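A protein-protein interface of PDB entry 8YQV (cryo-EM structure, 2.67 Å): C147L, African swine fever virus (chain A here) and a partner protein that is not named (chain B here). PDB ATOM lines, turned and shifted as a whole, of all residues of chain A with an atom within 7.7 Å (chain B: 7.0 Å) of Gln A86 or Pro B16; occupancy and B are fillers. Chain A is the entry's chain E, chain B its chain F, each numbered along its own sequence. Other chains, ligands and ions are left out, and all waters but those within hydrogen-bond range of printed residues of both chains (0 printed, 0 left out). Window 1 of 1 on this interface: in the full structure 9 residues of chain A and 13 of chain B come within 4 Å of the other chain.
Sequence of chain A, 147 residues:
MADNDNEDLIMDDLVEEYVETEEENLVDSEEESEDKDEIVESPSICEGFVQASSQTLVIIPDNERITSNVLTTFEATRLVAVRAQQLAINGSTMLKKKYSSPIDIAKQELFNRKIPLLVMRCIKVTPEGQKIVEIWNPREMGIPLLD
The side-chain carboxylate (OD1) of Asp B14 lies within salt-bridge range of the guanidinium group (NH1) of Arg B67 (3.6 Å).
NH2 of Arg A83 is in hydrogen-bond range of O of Ser A92 (3.1 Å).
The backbone carbonyl oxygen (O) of Asn B18 sits at hydrogen-bond distance from the side-chain hydroxyl (OG1) of Thr B21 (2.5 Å).
OG of Ser B65 lies close to N of Arg B67 (3.4 Å).
O of Pro B16 lies within hydrogen-bond range of SG of Cys B20, 3.4 Å away.
Among the printed residues, pairs that only touch across the chains: Gln A86 with Ile B59, Gln A85 with Ser B65, Asn A90 with Thr B17, Asn A90 with Asn B18, Ile A89 with Asp B15, Arg A83 with Thr B17, Gln A86 with Thr B17, Gln A85 with Gly B66, Gln A86 with Pro B16, Val A82 with Ile B59, Ile A89 with Asp B14 and Ile A89 with Ser B65.
Of the 18 printed residues of chain A, 6 touch a printed residue of chain B.
Among the printed residues, 14 pairs touch across the chains.
Among the printed residues, no Asp or Glu carboxylate lies within 4 Å of a Lys or Arg side-chain nitrogen of the other chain.
ND2 of Asn A90 is in hydrogen-bond range of OD1 of Asp B15, 2.6 Å away.
The backbone carbonyl oxygen of Gly B66 lies close to the side-chain amide nitrogen of Gln A86 (3.4 Å).
Printed residues of chain B within 4 Å of Arg A83: Thr B17 (3.8 Å).
Printed residues of chain B within 4 Å of Gln A85: Ser B65 and Gly B66.
Gln A86 touches just these residues of chain B: Pro B16, Thr B17, Ile B59 and Gly B66.
Leu A87 touches none of the printed residues of chain B.
Of chain A, only Gln A86 comes within 4 Å of Pro B16.
The nearest residue of chain A that does not touch Pro B16 is Ile A89 (5.0 Å).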
ATOM      1  N   LEU A  79     -21.220  -8.176  12.379  1.00  0.00           N
ATOM      2  CA  LEU A  79     -20.999  -6.747  12.573  1.00  0.00           C
ATOM      3  C   LEU A  79     -19.696  -6.301  11.934  1.00  0.00           C
ATOM      4  O   LEU A  79     -19.652  -5.275  11.250  1.00  0.00           O
ATOM      5  CB  LEU A  79     -20.984  -6.405  14.060  1.00  0.00           C
ATOM      6  CG  LEU A  79     -22.269  -6.360  14.869  1.00  0.00           C
ATOM      7  CD1 LEU A  79     -21.883  -6.300  16.304  1.00  0.00           C
ATOM      8  CD2 LEU A  79     -23.109  -5.166  14.519  1.00  0.00           C
ATOM      9  N   VAL A  80     -18.621  -7.063  12.143  1.00  0.00           N
ATOM     10  CA  VAL A  80     -17.341  -6.675  11.565  1.00  0.00           C
ATOM     11  C   VAL A  80     -17.379  -6.769  10.045  1.00  0.00           C
ATOM     12  O   VAL A  80     -16.825  -5.911   9.358  1.00  0.00           O
ATOM     13  CB  VAL A  80     -16.207  -7.515  12.175  1.00  0.00           C
ATOM     14  CG1 VAL A  80     -14.902  -7.234  11.480  1.00  0.00           C
ATOM     15  CG2 VAL A  80     -16.069  -7.199  13.640  1.00  0.00           C
ATOM     16  N   ALA A  81     -18.048  -7.781   9.489  1.00  0.00           N
ATOM     17  CA  ALA A  81     -18.139  -7.901   8.038  1.00  0.00           C
ATOM     18  C   ALA A  81     -18.920  -6.744   7.424  1.00  0.00           C
ATOM     19  O   ALA A  81     -18.487  -6.143   6.431  1.00  0.00           O
ATOM     20  CB  ALA A  81     -18.780  -9.236   7.670  1.00  0.00           C
ATOM     21  N   VAL A  82     -20.077  -6.416   8.004  1.00  0.00           N
ATOM     22  CA  VAL A  82     -20.885  -5.321   7.482  1.00  0.00           C
ATOM     23  C   VAL A  82     -20.133  -4.008   7.588  1.00  0.00           C
ATOM     24  O   VAL A  82     -20.097  -3.219   6.639  1.00  0.00           O
ATOM     25  CB  VAL A  82     -22.235  -5.255   8.217  1.00  0.00           C
ATOM     26  CG1 VAL A  82     -22.949  -3.970   7.891  1.00  0.00           C
ATOM     27  CG2 VAL A  82     -23.087  -6.435   7.846  1.00  0.00           C
ATOM     28  N   ARG A  83     -19.512  -3.753   8.739  1.00  0.00           N
ATOM     29  CA  ARG A  83     -18.785  -2.508   8.919  1.00  0.00           C
ATOM     30  C   ARG A  83     -17.579  -2.421   7.996  1.00  0.00           C
ATOM     31  O   ARG A  83     -17.268  -1.341   7.496  1.00  0.00           O
ATOM     32  CB  ARG A  83     -18.367  -2.367  10.376  1.00  0.00           C
ATOM     33  CG  ARG A  83     -17.673  -1.081  10.692  1.00  0.00           C
ATOM     34  CD  ARG A  83     -18.481   0.090  10.215  1.00  0.00           C
ATOM     35  NE  ARG A  83     -17.865   1.352  10.594  1.00  0.00           N
ATOM     36  CZ  ARG A  83     -18.019   2.481   9.924  1.00  0.00           C
ATOM     37  NH1 ARG A  83     -18.741   2.535   8.820  1.00  0.00           N
ATOM     38  NH2 ARG A  83     -17.430   3.584  10.372  1.00  0.00           N
ATOM     39  N   ALA A  84     -16.892  -3.535   7.752  1.00  0.00           N
ATOM     40  CA  ALA A  84     -15.764  -3.523   6.829  1.00  0.00           C
ATOM     41  C   ALA A  84     -16.210  -3.208   5.409  1.00  0.00           C
ATOM     42  O   ALA A  84     -15.550  -2.436   4.707  1.00  0.00           O
ATOM     43  CB  ALA A  84     -15.039  -4.862   6.881  1.00  0.00           C
ATOM     44  N   GLN A  85     -17.317  -3.798   4.958  1.00  0.00           N
ATOM     45  CA  GLN A  85     -17.798  -3.470   3.620  1.00  0.00           C
ATOM     46  C   GLN A  85     -18.236  -2.012   3.528  1.00  0.00           C
ATOM     47  O   GLN A  85     -17.964  -1.331   2.531  1.00  0.00           O
ATOM     48  CB  GLN A  85     -18.938  -4.397   3.221  1.00  0.00           C
ATOM     49  CG  GLN A  85     -19.410  -4.179   1.805  1.00  0.00           C
ATOM     50  CD  GLN A  85     -18.411  -4.645   0.779  1.00  0.00           C
ATOM     51  OE1 GLN A  85     -18.071  -5.820   0.718  1.00  0.00           O
ATOM     52  NE2 GLN A  85     -17.923  -3.719  -0.025  1.00  0.00           N
ATOM     53  N   GLN A  86     -18.911  -1.506   4.557  1.00  0.00           N
ATOM     54  CA  GLN A  86     -19.323  -0.110   4.534  1.00  0.00           C
ATOM     55  C   GLN A  86     -18.148   0.848   4.651  1.00  0.00           C
ATOM     56  O   GLN A  86     -18.267   2.001   4.228  1.00  0.00           O
ATOM     57  CB  GLN A  86     -20.328   0.155   5.645  1.00  0.00           C
ATOM     58  CG  GLN A  86     -21.642  -0.533   5.439  1.00  0.00           C
ATOM     59  CD  GLN A  86     -22.563  -0.325   6.596  1.00  0.00           C
ATOM     60  OE1 GLN A  86     -22.170   0.232   7.616  1.00  0.00           O
ATOM     61  NE2 GLN A  86     -23.801  -0.755   6.450  1.00  0.00           N
ATOM     62  N   LEU A  87     -17.034   0.415   5.235  1.00  0.00           N
ATOM     63  CA  LEU A  87     -15.807   1.199   5.177  1.00  0.00           C
ATOM     64  C   LEU A  87     -15.167   1.128   3.803  1.00  0.00           C
ATOM     65  O   LEU A  87     -14.533   2.092   3.368  1.00  0.00           O
ATOM     66  CB  LEU A  87     -14.814   0.717   6.230  1.00  0.00           C
ATOM     67  CG  LEU A  87     -15.086   1.207   7.644  1.00  0.00           C
ATOM     68  CD1 LEU A  87     -14.463   0.271   8.641  1.00  0.00           C
ATOM     69  CD2 LEU A  87     -14.553   2.606   7.816  1.00  0.00           C
ATOM     70  N   ALA A  88     -15.304  -0.005   3.120  1.00  0.00           N
ATOM     71  CA  ALA A  88     -14.914  -0.068   1.721  1.00  0.00           C
ATOM     72  C   ALA A  88     -15.747   0.870   0.864  1.00  0.00           C
ATOM     73  O   ALA A  88     -15.293   1.275  -0.208  1.00  0.00           O
ATOM     74  CB  ALA A  88     -15.027  -1.496   1.197  1.00  0.00           C
ATOM     75  N   ILE A  89     -16.954   1.217   1.307  1.00  0.00           N
ATOM     76  CA  ILE A  89     -17.767   2.187   0.574  1.00  0.00           C
ATOM     77  C   ILE A  89     -17.369   3.617   0.932  1.00  0.00           C
ATOM     78  O   ILE A  89     -16.986   4.402   0.059  1.00  0.00           O
ATOM     79  CB  ILE A  89     -19.265   1.941   0.825  1.00  0.00           C
ATOM     80  CG1 ILE A  89     -19.719   0.649   0.148  1.00  0.00           C
ATOM     81  CG2 ILE A  89     -20.085   3.109   0.317  1.00  0.00           C
ATOM     82  CD1 ILE A  89     -21.133   0.235   0.514  1.00  0.00           C
ATOM     83  N   ASN A  90     -17.461   3.985   2.212  1.00  0.00           N
ATOM     84  CA  ASN A  90     -17.193   5.371   2.627  1.00  0.00           C
ATOM     85  C   ASN A  90     -15.749   5.591   3.069  1.00  0.00           C
ATOM     86  O   ASN A  90     -15.011   6.361   2.450  1.00  0.00           O
ATOM     87  CB  ASN A  90     -18.139   5.784   3.755  1.00  0.00           C
ATOM     88  CG  ASN A  90     -19.183   6.773   3.305  1.00  0.00           C
ATOM     89  OD1 ASN A  90     -18.936   7.593   2.425  1.00  0.00           O
ATOM     90  ND2 ASN A  90     -20.350   6.726   3.929  1.00  0.00           N
ATOM     91  N   GLY A  91     -15.335   4.919   4.134  1.00  0.00           N
ATOM     92  CA  GLY A  91     -14.053   5.185   4.743  1.00  0.00           C
ATOM     93  C   GLY A  91     -14.081   6.154   5.904  1.00  0.00           C
ATOM     94  O   GLY A  91     -13.023   6.440   6.472  1.00  0.00           O
ATOM     95  N   SER A  92     -15.248   6.666   6.278  1.00  0.00           N
ATOM     96  CA  SER A  92     -15.352   7.604   7.389  1.00  0.00           C
ATOM     97  C   SER A  92     -15.495   6.835   8.694  1.00  0.00           C
ATOM     98  O   SER A  92     -16.432   6.046   8.855  1.00  0.00           O
ATOM     99  CB  SER A  92     -16.539   8.539   7.181  1.00  0.00           C
ATOM    100  OG  SER A  92     -16.702   9.410   8.284  1.00  0.00           O
ATOM    101  N   PRO A 102      -9.970  -2.155   5.491  1.00  0.00           N
ATOM    102  CA  PRO A 102     -11.285  -2.026   6.128  1.00  0.00           C
ATOM    103  C   PRO A 102     -11.491  -3.020   7.248  1.00  0.00           C
ATOM    104  O   PRO A 102     -12.176  -2.709   8.225  1.00  0.00           O
ATOM    105  CB  PRO A 102     -12.264  -2.282   4.975  1.00  0.00           C
ATOM    106  CG  PRO A 102     -11.454  -2.232   3.743  1.00  0.00           C
ATOM    107  CD  PRO A 102     -10.084  -2.650   4.115  1.00  0.00           C
ATOM    108  N   ILE A 115     -18.274   1.073  16.875  1.00  0.00           N
ATOM    109  CA  ILE A 115     -18.932   0.579  15.669  1.00  0.00           C
ATOM    110  C   ILE A 115     -20.360   1.115  15.612  1.00  0.00           C
ATOM    111  O   ILE A 115     -21.144   0.906  16.545  1.00  0.00           O
ATOM    112  CB  ILE A 115     -18.869  -0.958  15.622  1.00  0.00           C
ATOM    113  CG1 ILE A 115     -19.501  -1.510  14.354  1.00  0.00           C
ATOM    114  CG2 ILE A 115     -19.501  -1.579  16.851  1.00  0.00           C
ATOM    115  CD1 ILE A 115     -19.083  -2.917  14.070  1.00  0.00           C
ATOM    116  N   PRO A 116     -20.742   1.820  14.551  1.00  0.00           N
ATOM    117  CA  PRO A 116     -22.039   2.505  14.500  1.00  0.00           C
ATOM    118  C   PRO A 116     -23.186   1.633  13.993  1.00  0.00           C
ATOM    119  O   PRO A 116     -23.914   2.006  13.076  1.00  0.00           O
ATOM    120  CB  PRO A 116     -21.762   3.665  13.543  1.00  0.00           C
ATOM    121  CG  PRO A 116     -20.797   3.081  12.587  1.00  0.00           C
ATOM    122  CD  PRO A 116     -19.933   2.119  13.361  1.00  0.00           C
ATOM    123  N   LEU A 117     -23.355   0.466  14.603  1.00  0.00           N
ATOM    124  CA  LEU A 117     -24.385  -0.473  14.199  1.00  0.00           C
ATOM    125  C   LEU A 117     -25.135  -0.954  15.429  1.00  0.00           C
ATOM    126  O   LEU A 117     -24.653  -0.843  16.554  1.00  0.00           O
ATOM    127  CB  LEU A 117     -23.796  -1.668  13.444  1.00  0.00           C
ATOM    128  CG  LEU A 117     -23.036  -1.405  12.145  1.00  0.00           C
ATOM    129  CD1 LEU A 117     -22.356  -2.668  11.673  1.00  0.00           C
ATOM    130  CD2 LEU A 117     -23.962  -0.894  11.084  1.00  0.00           C
ATOM    131  N   ILE B  13     -30.547   1.940  -0.114  1.00  0.00           N
ATOM    132  CA  ILE B  13     -29.559   2.931   0.281  1.00  0.00           C
ATOM    133  C   ILE B  13     -28.194   2.388  -0.108  1.00  0.00           C
ATOM    134  O   ILE B  13     -27.770   1.340   0.388  1.00  0.00           O
ATOM    135  CB  ILE B  13     -29.626   3.233   1.781  1.00  0.00           C
ATOM    136  CG1 ILE B  13     -30.928   3.949   2.121  1.00  0.00           C
ATOM    137  CG2 ILE B  13     -28.455   4.071   2.191  1.00  0.00           C
ATOM    138  CD1 ILE B  13     -31.964   3.070   2.700  1.00  0.00           C
ATOM    139  N   ASP B  14     -27.504   3.098  -0.998  1.00  0.00           N
ATOM    140  CA  ASP B  14     -26.200   2.659  -1.469  1.00  0.00           C
ATOM    141  C   ASP B  14     -25.064   3.069  -0.543  1.00  0.00           C
ATOM    142  O   ASP B  14     -23.944   2.584  -0.715  1.00  0.00           O
ATOM    143  CB  ASP B  14     -25.937   3.211  -2.869  1.00  0.00           C
ATOM    144  CG  ASP B  14     -26.743   2.501  -3.937  1.00  0.00           C
ATOM    145  OD1 ASP B  14     -27.482   1.551  -3.605  1.00  0.00           O
ATOM    146  OD2 ASP B  14     -26.637   2.895  -5.116  1.00  0.00           O
ATOM    147  N   ASP B  15     -25.325   3.942   0.427  1.00  0.00           N
ATOM    148  CA  ASP B  15     -24.298   4.390   1.366  1.00  0.00           C
ATOM    149  C   ASP B  15     -24.962   4.637   2.704  1.00  0.00           C
ATOM    150  O   ASP B  15     -25.274   5.780   3.057  1.00  0.00           O
ATOM    151  CB  ASP B  15     -23.598   5.652   0.871  1.00  0.00           C
ATOM    152  CG  ASP B  15     -22.366   5.988   1.676  1.00  0.00           C
ATOM    153  OD1 ASP B  15     -21.980   5.181   2.543  1.00  0.00           O
ATOM    154  OD2 ASP B  15     -21.786   7.066   1.448  1.00  0.00           O
ATOM    155  N   PRO B  16     -25.206   3.582   3.481  1.00  0.00           N
ATOM    156  CA  PRO B  16     -25.984   3.755   4.717  1.00  0.00           C
ATOM    157  C   PRO B  16     -25.358   4.713   5.712  1.00  0.00           C
ATOM    158  O   PRO B  16     -26.089   5.450   6.385  1.00  0.00           O
ATOM    159  CB  PRO B  16     -26.061   2.331   5.276  1.00  0.00           C
ATOM    160  CG  PRO B  16     -25.806   1.451   4.116  1.00  0.00           C
ATOM    161  CD  PRO B  16     -24.832   2.178   3.265  1.00  0.00           C
ATOM    162  N   THR B  17     -24.029   4.731   5.819  1.00  0.00           N
ATOM    163  CA  THR B  17     -23.378   5.587   6.803  1.00  0.00           C
ATOM    164  C   THR B  17     -23.632   7.059   6.519  1.00  0.00           C
ATOM    165  O   THR B  17     -23.848   7.840   7.450  1.00  0.00           O
ATOM    166  CB  THR B  17     -21.879   5.305   6.832  1.00  0.00           C
ATOM    167  OG1 THR B  17     -21.660   3.893   6.860  1.00  0.00           O
ATOM    168  CG2 THR B  17     -21.258   5.915   8.061  1.00  0.00           C
ATOM    169  N   ASN B  18     -23.600   7.456   5.249  1.00  0.00           N
ATOM    170  CA  ASN B  18     -23.932   8.827   4.887  1.00  0.00           C
ATOM    171  C   ASN B  18     -25.423   9.092   5.016  1.00  0.00           C
ATOM    172  O   ASN B  18     -25.825  10.139   5.532  1.00  0.00           O
ATOM    173  CB  ASN B  18     -23.472   9.118   3.461  1.00  0.00           C
ATOM    174  CG  ASN B  18     -23.569  10.583   3.108  1.00  0.00           C
ATOM    175  OD1 ASN B  18     -23.791  11.428   3.970  1.00  0.00           O
ATOM    176  ND2 ASN B  18     -23.422  10.889   1.828  1.00  0.00           N
ATOM    177  N   PHE B  19     -26.253   8.154   4.559  1.00  0.00           N
ATOM    178  CA  PHE B  19     -27.698   8.355   4.586  1.00  0.00           C
ATOM    179  C   PHE B  19     -28.199   8.589   6.001  1.00  0.00           C
ATOM    180  O   PHE B  19     -29.106   9.396   6.218  1.00  0.00           O
ATOM    181  CB  PHE B  19     -28.399   7.149   3.966  1.00  0.00           C
ATOM    182  CG  PHE B  19     -29.885   7.314   3.810  1.00  0.00           C
ATOM    183  CD1 PHE B  19     -30.423   7.789   2.633  1.00  0.00           C
ATOM    184  CD2 PHE B  19     -30.745   6.983   4.842  1.00  0.00           C
ATOM    185  CE1 PHE B  19     -31.785   7.932   2.489  1.00  0.00           C
ATOM    186  CE2 PHE B  19     -32.103   7.131   4.704  1.00  0.00           C
ATOM    187  CZ  PHE B  19     -32.624   7.604   3.528  1.00  0.00           C
ATOM    188  N   CYS B  20     -27.623   7.895   6.977  1.00  0.00           N
ATOM    189  CA  CYS B  20     -28.116   7.986   8.344  1.00  0.00           C
ATOM    190  C   CYS B  20     -27.648   9.237   9.077  1.00  0.00           C
ATOM    191  O   CYS B  20     -28.079   9.456  10.211  1.00  0.00           O
ATOM    192  CB  CYS B  20     -27.712   6.737   9.130  1.00  0.00           C
ATOM    193  SG  CYS B  20     -28.639   5.261   8.679  1.00  0.00           S
ATOM    194  N   THR B  21     -26.786  10.057   8.474  1.00  0.00           N
ATOM    195  CA  THR B  21     -26.413  11.317   9.109  1.00  0.00           C
ATOM    196  C   THR B  21     -27.590  12.286   9.169  1.00  0.00           C
ATOM    197  O   THR B  21     -27.669  13.103  10.091  1.00  0.00           O
ATOM    198  CB  THR B  21     -25.237  11.960   8.376  1.00  0.00           C
ATOM    199  OG1 THR B  21     -25.593  12.196   7.011  1.00  0.00           O
ATOM    200  CG2 THR B  21     -24.025  11.058   8.424  1.00  0.00           C
ATOM    201  N   CYS B  57     -32.888   1.514   9.103  1.00  0.00           N
ATOM    202  CA  CYS B  57     -32.111   1.215   7.905  1.00  0.00           C
ATOM    203  C   CYS B  57     -31.514  -0.176   8.068  1.00  0.00           C
ATOM    204  O   CYS B  57     -30.430  -0.351   8.617  1.00  0.00           O
ATOM    205  CB  CYS B  57     -31.037   2.268   7.676  1.00  0.00           C
ATOM    206  SG  CYS B  57     -30.101   2.042   6.148  1.00  0.00           S
ATOM    207  N   PHE B  58     -32.243  -1.181   7.604  1.00  0.00           N
ATOM    208  CA  PHE B  58     -31.756  -2.547   7.650  1.00  0.00           C
ATOM    209  C   PHE B  58     -30.629  -2.741   6.649  1.00  0.00           C
ATOM    210  O   PHE B  58     -30.614  -2.138   5.578  1.00  0.00           O
ATOM    211  CB  PHE B  58     -32.873  -3.537   7.335  1.00  0.00           C
ATOM    212  CG  PHE B  58     -34.081  -3.390   8.200  1.00  0.00           C
ATOM    213  CD1 PHE B  58     -34.070  -3.834   9.504  1.00  0.00           C
ATOM    214  CD2 PHE B  58     -35.238  -2.832   7.701  1.00  0.00           C
ATOM    215  CE1 PHE B  58     -35.179  -3.709  10.298  1.00  0.00           C
ATOM    216  CE2 PHE B  58     -36.352  -2.709   8.493  1.00  0.00           C
ATOM    217  CZ  PHE B  58     -36.320  -3.148   9.793  1.00  0.00           C
ATOM    218  N   ILE B  59     -29.699  -3.599   6.997  1.00  0.00           N
ATOM    219  CA  ILE B  59     -28.616  -3.975   6.100  1.00  0.00           C
ATOM    220  C   ILE B  59     -29.062  -5.183   5.296  1.00  0.00           C
ATOM    221  O   ILE B  59     -29.556  -6.163   5.858  1.00  0.00           O
ATOM    222  CB  ILE B  59     -27.329  -4.268   6.890  1.00  0.00           C
ATOM    223  CG1 ILE B  59     -27.011  -3.109   7.827  1.00  0.00           C
ATOM    224  CG2 ILE B  59     -26.177  -4.508   5.956  1.00  0.00           C
ATOM    225  CD1 ILE B  59     -26.856  -1.802   7.131  1.00  0.00           C
ATOM    226  N   SER B  65     -23.181  -6.900  -0.339  1.00  0.00           N
ATOM    227  CA  SER B  65     -22.999  -5.535  -0.806  1.00  0.00           C
ATOM    228  C   SER B  65     -22.790  -4.528   0.312  1.00  0.00           C
ATOM    229  O   SER B  65     -22.250  -3.449   0.055  1.00  0.00           O
ATOM    230  CB  SER B  65     -24.202  -5.104  -1.637  1.00  0.00           C
ATOM    231  OG  SER B  65     -25.379  -5.141  -0.859  1.00  0.00           O
ATOM    232  N   GLY B  66     -23.195  -4.846   1.537  1.00  0.00           N
ATOM    233  CA  GLY B  66     -23.087  -3.891   2.619  1.00  0.00           C
ATOM    234  C   GLY B  66     -24.047  -2.739   2.520  1.00  0.00           C
ATOM    235  O   GLY B  66     -23.860  -1.729   3.200  1.00  0.00           O
ATOM    236  N   ARG B  67     -25.083  -2.871   1.705  1.00  0.00           N
ATOM    237  CA  ARG B  67     -26.013  -1.803   1.384  1.00  0.00           C
ATOM    238  C   ARG B  67     -27.225  -1.889   2.297  1.00  0.00           C
ATOM    239  O   ARG B  67     -27.472  -2.910   2.939  1.00  0.00           O
ATOM    240  CB  ARG B  67     -26.443  -1.897  -0.078  1.00  0.00           C
ATOM    241  CG  ARG B  67     -25.618  -1.051  -1.013  1.00  0.00           C
ATOM    242  CD  ARG B  67     -26.170  -1.103  -2.416  1.00  0.00           C
ATOM    243  NE  ARG B  67     -26.457  -2.467  -2.837  1.00  0.00           N
ATOM    244  CZ  ARG B  67     -27.404  -2.800  -3.702  1.00  0.00           C
ATOM    245  NH1 ARG B  67     -28.189  -1.888  -4.250  1.00  0.00           N
ATOM    246  NH2 ARG B  67     -27.573  -4.079  -4.021  1.00  0.00           N
ATOM    247  N   GLY B  68     -27.981  -0.802   2.356  1.00  0.00           N
ATOM    248  CA  GLY B  68     -29.112  -0.763   3.255  1.00  0.00           C
ATOM    249  C   GLY B  68     -30.444  -0.715   2.545  1.00  0.00           C
ATOM    250  O   GLY B  68     -30.494  -0.532   1.330  1.00  0.00           O
ATOM    251  N   TYR B  69     -31.532  -0.876   3.284  1.00  0.00           N
ATOM    252  CA  TYR B  69     -32.853  -0.652   2.724  1.00  0.00           C
ATOM    253  C   TYR B  69     -33.765  -0.153   3.828  1.00  0.00           C
ATOM    254  O   TYR B  69     -33.554  -0.432   5.008  1.00  0.00           O
ATOM    255  CB  TYR B  69     -33.416  -1.910   2.057  1.00  0.00           C
ATOM    256  CG  TYR B  69     -33.726  -3.059   2.984  1.00  0.00           C
ATOM    257  CD1 TYR B  69     -32.751  -3.976   3.334  1.00  0.00           C
ATOM    258  CD2 TYR B  69     -34.998  -3.238   3.490  1.00  0.00           C
ATOM    259  CE1 TYR B  69     -33.033  -5.028   4.166  1.00  0.00           C
ATOM    260  CE2 TYR B  69     -35.285  -4.284   4.324  1.00  0.00           C
ATOM    261  CZ  TYR B  69     -34.300  -5.177   4.656  1.00  0.00           C
ATOM    262  OH  TYR B  69     -34.589  -6.226   5.488  1.00  0.00           O
